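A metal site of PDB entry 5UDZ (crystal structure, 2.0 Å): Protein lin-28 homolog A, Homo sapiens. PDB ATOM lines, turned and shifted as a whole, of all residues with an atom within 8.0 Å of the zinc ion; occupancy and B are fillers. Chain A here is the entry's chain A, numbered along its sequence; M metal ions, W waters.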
ATOM      1  N   VAL A  85       8.540 -19.604  15.460  1.00  0.00           N
ATOM      2  CA  VAL A  85       8.350 -18.480  14.548  1.00  0.00           C
ATOM      3  C   VAL A  85       7.663 -18.928  13.251  1.00  0.00           C
ATOM      4  O   VAL A  85       7.347 -20.116  13.077  1.00  0.00           O
ATOM      5  CB  VAL A  85       9.690 -17.819  14.213  1.00  0.00           C
ATOM      6  CG1 VAL A  85      10.447 -17.482  15.510  1.00  0.00           C
ATOM      7  CG2 VAL A  85      10.528 -18.719  13.309  1.00  0.00           C
ATOM      8  N   PHE A  86       7.423 -17.986  12.330  1.00  0.00           N
ATOM      9  CA  PHE A  86       6.686 -18.292  11.108  1.00  0.00           C
ATOM     10  C   PHE A  86       7.550 -19.165  10.207  1.00  0.00           C
ATOM     11  O   PHE A  86       8.788 -19.079  10.247  1.00  0.00           O
ATOM     12  CB  PHE A  86       6.277 -17.019  10.347  1.00  0.00           C
ATOM     13  CG  PHE A  86       5.322 -16.147  11.096  1.00  0.00           C
ATOM     14  CD1 PHE A  86       4.035 -16.592  11.399  1.00  0.00           C
ATOM     15  CD2 PHE A  86       5.692 -14.893  11.495  1.00  0.00           C
ATOM     16  CE1 PHE A  86       3.169 -15.790  12.086  1.00  0.00           C
ATOM     17  CE2 PHE A  86       4.824 -14.067  12.202  1.00  0.00           C
ATOM     18  CZ  PHE A  86       3.557 -14.517  12.483  1.00  0.00           C
ATOM     19  N   ARG A  99      11.537 -10.892   5.001  1.00  0.00           N
ATOM     20  CA  ARG A  99      10.966 -11.362   6.262  1.00  0.00           C
ATOM     21  C   ARG A  99      11.698 -10.743   7.454  1.00  0.00           C
ATOM     22  O   ARG A  99      12.902 -10.493   7.387  1.00  0.00           O
ATOM     23  CB  ARG A  99      11.077 -12.879   6.335  1.00  0.00           C
ATOM     24  CG  ARG A  99      10.653 -13.610   5.054  1.00  0.00           C
ATOM     25  CD  ARG A  99      10.612 -15.151   5.229  1.00  0.00           C
ATOM     26  NE  ARG A  99      11.912 -15.717   5.601  1.00  0.00           N
ATOM     27  CZ  ARG A  99      12.860 -16.062   4.722  1.00  0.00           C
ATOM     28  NH1 ARG A  99      14.010 -16.570   5.145  1.00  0.00           N
ATOM     29  NH2 ARG A  99      12.688 -15.900   3.413  1.00  0.00           N
ATOM     30  N   CYS A 100      10.989 -10.525   8.547  1.00  0.00           N
ATOM     31  CA  CYS A 100      11.647 -10.109   9.784  1.00  0.00           C
ATOM     32  C   CYS A 100      12.729 -11.115  10.180  1.00  0.00           C
ATOM     33  O   CYS A 100      12.441 -12.312  10.269  1.00  0.00           O
ATOM     34  CB  CYS A 100      10.602  -9.999  10.896  1.00  0.00           C
ATOM     35  SG  CYS A 100      11.307  -9.771  12.519  1.00  0.00           S
ATOM     36  N   TYR A 101      13.957 -10.660  10.419  1.00  0.00           N
ATOM     37  CA  TYR A 101      15.034 -11.590  10.788  1.00  0.00           C
ATOM     38  C   TYR A 101      14.686 -12.354  12.039  1.00  0.00           C
ATOM     39  O   TYR A 101      15.173 -13.459  12.253  1.00  0.00           O
ATOM     40  CB  TYR A 101      16.359 -10.857  11.051  1.00  0.00           C
ATOM     41  CG  TYR A 101      17.005 -10.201   9.861  1.00  0.00           C
ATOM     42  CD1 TYR A 101      16.949 -10.766   8.589  1.00  0.00           C
ATOM     43  CD2 TYR A 101      17.671  -8.989  10.009  1.00  0.00           C
ATOM     44  CE1 TYR A 101      17.557 -10.151   7.504  1.00  0.00           C
ATOM     45  CE2 TYR A 101      18.287  -8.358   8.922  1.00  0.00           C
ATOM     46  CZ  TYR A 101      18.227  -8.949   7.681  1.00  0.00           C
ATOM     47  OH  TYR A 101      18.845  -8.315   6.637  1.00  0.00           O
ATOM     48  N   ASN A 102      13.848 -11.776  12.889  1.00  0.00           N
ATOM     49  CA  ASN A 102      13.637 -12.364  14.216  1.00  0.00           C
ATOM     50  C   ASN A 102      12.515 -13.404  14.236  1.00  0.00           C
ATOM     51  O   ASN A 102      12.672 -14.443  14.871  1.00  0.00           O
ATOM     52  CB  ASN A 102      13.351 -11.264  15.223  1.00  0.00           C
ATOM     53  CG  ASN A 102      13.411 -11.737  16.654  1.00  0.00           C
ATOM     54  OD1 ASN A 102      14.416 -12.277  17.094  1.00  0.00           O
ATOM     55  ND2 ASN A 102      12.334 -11.522  17.388  1.00  0.00           N
ATOM     56  N   CYS A 103      11.395 -13.107  13.569  1.00  0.00           N
ATOM     57  CA  CYS A 103      10.227 -13.987  13.611  1.00  0.00           C
ATOM     58  C   CYS A 103       9.780 -14.499  12.253  1.00  0.00           C
ATOM     59  O   CYS A 103       8.855 -15.294  12.197  1.00  0.00           O
ATOM     60  CB  CYS A 103       9.033 -13.293  14.289  1.00  0.00           C
ATOM     61  SG  CYS A 103       8.207 -12.045  13.280  1.00  0.00           S
ATOM     62  N   GLY A 104      10.392 -14.019  11.174  1.00  0.00           N
ATOM     63  CA  GLY A 104      10.039 -14.428   9.815  1.00  0.00           C
ATOM     64  C   GLY A 104       8.809 -13.753   9.231  1.00  0.00           C
ATOM     65  O   GLY A 104       8.406 -14.070   8.114  1.00  0.00           O
ATOM     66  N   GLY A 105       8.197 -12.863   9.990  1.00  0.00           N
ATOM     67  CA  GLY A 105       7.026 -12.122   9.552  1.00  0.00           C
ATOM     68  C   GLY A 105       7.238 -11.190   8.362  1.00  0.00           C
ATOM     69  O   GLY A 105       8.306 -10.625   8.135  1.00  0.00           O
ATOM     70  N   LEU A 106       6.153 -11.001   7.626  1.00  0.00           N
ATOM     71  CA  LEU A 106       6.182 -10.273   6.372  1.00  0.00           C
ATOM     72  C   LEU A 106       5.912  -8.767   6.492  1.00  0.00           C
ATOM     73  O   LEU A 106       6.111  -8.043   5.501  1.00  0.00           O
ATOM     74  CB  LEU A 106       5.152 -10.899   5.444  1.00  0.00           C
ATOM     75  CG  LEU A 106       5.623 -11.991   4.484  1.00  0.00           C
ATOM     76  CD1 LEU A 106       6.627 -12.932   5.105  1.00  0.00           C
ATOM     77  CD2 LEU A 106       4.413 -12.730   3.930  1.00  0.00           C
ATOM     78  N   ASP A 107       5.477  -8.283   7.667  1.00  0.00           N
ATOM     79  CA  ASP A 107       4.982  -6.890   7.781  1.00  0.00           C
ATOM     80  C   ASP A 107       5.875  -5.962   8.643  1.00  0.00           C
ATOM     81  O   ASP A 107       5.450  -4.878   9.026  1.00  0.00           O
ATOM     82  CB  ASP A 107       3.548  -6.864   8.315  1.00  0.00           C
ATOM     83  CG  ASP A 107       3.404  -7.529   9.696  1.00  0.00           C
ATOM     84  OD1 ASP A 107       4.433  -7.915  10.283  1.00  0.00           O
ATOM     85  OD2 ASP A 107       2.258  -7.658  10.190  1.00  0.00           O
ATOM     86  N   HIS A 108       7.079  -6.406   8.965  1.00  0.00           N
ATOM     87  CA  HIS A 108       7.962  -5.612   9.798  1.00  0.00           C
ATOM     88  C   HIS A 108       9.363  -6.156   9.736  1.00  0.00           C
ATOM     89  O   HIS A 108       9.596  -7.253   9.186  1.00  0.00           O
ATOM     90  CB  HIS A 108       7.466  -5.611  11.258  1.00  0.00           C
ATOM     91  CG  HIS A 108       7.554  -6.939  11.947  1.00  0.00           C
ATOM     92  ND1 HIS A 108       6.532  -7.872  11.916  1.00  0.00           N
ATOM     93  CD2 HIS A 108       8.541  -7.497  12.702  1.00  0.00           C
ATOM     94  CE1 HIS A 108       6.891  -8.945  12.588  1.00  0.00           C
ATOM     95  NE2 HIS A 108       8.097  -8.737  13.087  1.00  0.00           N
ATOM     96  N   HIS A 109      10.296  -5.399  10.308  1.00  0.00           N
ATOM     97  CA  HIS A 109      11.699  -5.787  10.372  1.00  0.00           C
ATOM     98  C   HIS A 109      12.102  -5.947  11.806  1.00  0.00           C
ATOM     99  O   HIS A 109      11.337  -5.598  12.690  1.00  0.00           O
ATOM    100  CB  HIS A 109      12.576  -4.767   9.654  1.00  0.00           C
ATOM    101  CG  HIS A 109      12.585  -4.957   8.165  1.00  0.00           C
ATOM    102  ND1 HIS A 109      13.378  -4.201   7.327  1.00  0.00           N
ATOM    103  CD2 HIS A 109      11.934  -5.842   7.379  1.00  0.00           C
ATOM    104  CE1 HIS A 109      13.192  -4.591   6.080  1.00  0.00           C
ATOM    105  NE2 HIS A 109      12.327  -5.595   6.077  1.00  0.00           N
ATOM    106  N   ALA A 110      13.283  -6.525  12.035  1.00  0.00           N
ATOM    107  CA  ALA A 110      13.666  -7.023  13.354  1.00  0.00           C
ATOM    108  C   ALA A 110      13.619  -5.931  14.436  1.00  0.00           C
ATOM    109  O   ALA A 110      13.293  -6.210  15.581  1.00  0.00           O
ATOM    110  CB  ALA A 110      15.045  -7.620  13.305  1.00  0.00           C
ATOM    111  N   LYS A 111      13.977  -4.712  14.064  1.00  0.00           N
ATOM    112  CA  LYS A 111      13.970  -3.603  15.022  1.00  0.00           C
ATOM    113  C   LYS A 111      12.560  -3.357  15.562  1.00  0.00           C
ATOM    114  O   LYS A 111      12.392  -3.007  16.731  1.00  0.00           O
ATOM    115  CB  LYS A 111      14.526  -2.347  14.353  1.00  0.00           C
ATOM    116  CG  LYS A 111      14.563  -1.109  15.225  1.00  0.00           C
ATOM    117  CD  LYS A 111      14.983   0.118  14.416  1.00  0.00           C
ATOM    118  CE  LYS A 111      15.085   1.389  15.275  1.00  0.00           C
ATOM    119  NZ  LYS A 111      13.752   1.960  15.672  1.00  0.00           N
ATOM    120  N   GLU A 112      11.540  -3.535  14.710  1.00  0.00           N
ATOM    121  CA  GLU A 112      10.167  -3.314  15.130  1.00  0.00           C
ATOM    122  C   GLU A 112       9.484  -4.571  15.720  1.00  0.00           C
ATOM    123  O   GLU A 112       8.297  -4.530  16.021  1.00  0.00           O
ATOM    124  CB  GLU A 112       9.296  -2.816  13.963  1.00  0.00           C
ATOM    125  CG  GLU A 112       9.956  -1.892  12.923  1.00  0.00           C
ATOM    126  CD  GLU A 112       9.218  -1.951  11.562  1.00  0.00           C
ATOM    127  OE1 GLU A 112       9.862  -2.298  10.534  1.00  0.00           O
ATOM    128  OE2 GLU A 112       7.996  -1.659  11.512  1.00  0.00           O
ATOM    129  N   CYS A 113      10.220  -5.675  15.858  1.00  0.00           N
ATOM    130  CA  CYS A 113       9.566  -6.958  16.186  1.00  0.00           C
ATOM    131  C   CYS A 113       9.018  -6.970  17.607  1.00  0.00           C
ATOM    132  O   CYS A 113       9.723  -6.629  18.565  1.00  0.00           O
ATOM    133  CB  CYS A 113      10.519  -8.157  15.968  1.00  0.00           C
ATOM    134  SG  CYS A 113       9.699  -9.808  16.055  1.00  0.00           S
ATOM    135  N   LYS A 114       7.781  -7.406  17.751  1.00  0.00           N
ATOM    136  CA  LYS A 114       7.121  -7.397  19.069  1.00  0.00           C
ATOM    137  C   LYS A 114       7.386  -8.638  19.897  1.00  0.00           C
ATOM    138  O   LYS A 114       6.972  -8.701  21.039  1.00  0.00           O
ATOM    139  CB  LYS A 114       5.609  -7.174  18.904  1.00  0.00           C
ATOM    140  CG  LYS A 114       5.264  -5.740  18.459  1.00  0.00           C
ATOM    141  CD  LYS A 114       3.880  -5.608  17.828  1.00  0.00           C
ATOM    142  CE  LYS A 114       3.753  -6.332  16.454  1.00  0.00           C
ATOM    143  NZ  LYS A 114       4.764  -5.915  15.413  1.00  0.00           N
ATOM    144  N   LEU A 115       8.085  -9.611  19.327  1.00  0.00           N
ATOM    145  CA  LEU A 115       8.505 -10.773  20.083  1.00  0.00           C
ATOM    146  C   LEU A 115       9.921 -10.552  20.564  1.00  0.00           C
ATOM    147  O   LEU A 115      10.674  -9.774  19.961  1.00  0.00           O
ATOM    148  CB  LEU A 115       8.415 -12.008  19.199  1.00  0.00           C
ATOM    149  CG  LEU A 115       7.010 -12.264  18.636  1.00  0.00           C
ATOM    150  CD1 LEU A 115       6.972 -13.495  17.770  1.00  0.00           C
ATOM    151  CD2 LEU A 115       6.000 -12.403  19.785  1.00  0.00           C
ATOM    152  N   PRO A 116      10.301 -11.245  21.646  1.00  0.00           N
ATOM    153  CA  PRO A 116      11.666 -11.122  22.174  1.00  0.00           C
ATOM    154  C   PRO A 116      12.728 -11.684  21.212  1.00  0.00           C
ATOM    155  O   PRO A 116      12.351 -12.439  20.294  1.00  0.00           O
ATOM    156  CB  PRO A 116      11.625 -11.952  23.438  1.00  0.00           C
ATOM    157  CG  PRO A 116      10.562 -12.971  23.176  1.00  0.00           C
ATOM    158  CD  PRO A 116       9.538 -12.291  22.332  1.00  0.00           C
ATOM    159  N   GLN A 118      15.056 -13.861  19.212  1.00  0.00           N
ATOM    160  CA  GLN A 118      15.086 -15.311  18.990  1.00  0.00           C
ATOM    161  C   GLN A 118      16.508 -15.694  18.584  1.00  0.00           C
ATOM    162  O   GLN A 118      17.299 -14.819  18.184  1.00  0.00           O
ATOM    163  CB  GLN A 118      14.139 -15.677  17.826  1.00  0.00           C
ATOM    164  CG  GLN A 118      12.669 -15.260  18.046  1.00  0.00           C
ATOM    165  CD  GLN A 118      12.012 -16.064  19.131  1.00  0.00           C
ATOM    166  OE1 GLN A 118      11.866 -17.284  19.002  1.00  0.00           O
ATOM    167  NE2 GLN A 118      11.665 -15.414  20.228  1.00  0.00           N
HETATM  168 ZN    ZN M   1       9.389 -10.070  13.841  1.00  0.00          ZN
HETATM  169  O   HOH W   1       6.426 -10.989  14.974  1.00  0.00           O
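The side-chain carboxylate (OD1) of Asp 107 sits at hydrogen-bond distance from a ring nitrogen (ND1) of His 108 (2.7 Å). The side-chain amide nitrogen (ND2) of Asn 102 lies close to the side-chain sulfur (SG) of Cys 113 (3.4 Å). N of Leu 115 sits close to SG of Cys 113 (3.7 Å). SG of Cys 100 sits close to N of Asn 102 (3.3 Å). The backbone NH (N) of Cys 100 lies within hydrogen-bond range of the backbone carbonyl oxygen (O) of Gly 105 (2.7 Å). The side-chain sulfur of Cys 103 sits close to the backbone NH of Gly 105. N of Phe 86 is in hydrogen-bond range of O of Cys 103 (3.1 Å).
Within 4 Å of the zinc ion: Cys 100, Cys 103, His 108 and Cys 113.
NE2 of His 108 is bound to the zinc ion (2.0 Å). The zinc ion is bound by the side-chain sulfur (SG) of Cys 113 (2.3 Å). The side-chain sulfur (SG) of Cys 100 binds the zinc ion (2.3 Å). SG of Cys 103 binds the zinc ion (2.4 Å). The zinc ion has four donor atoms within binding distance.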
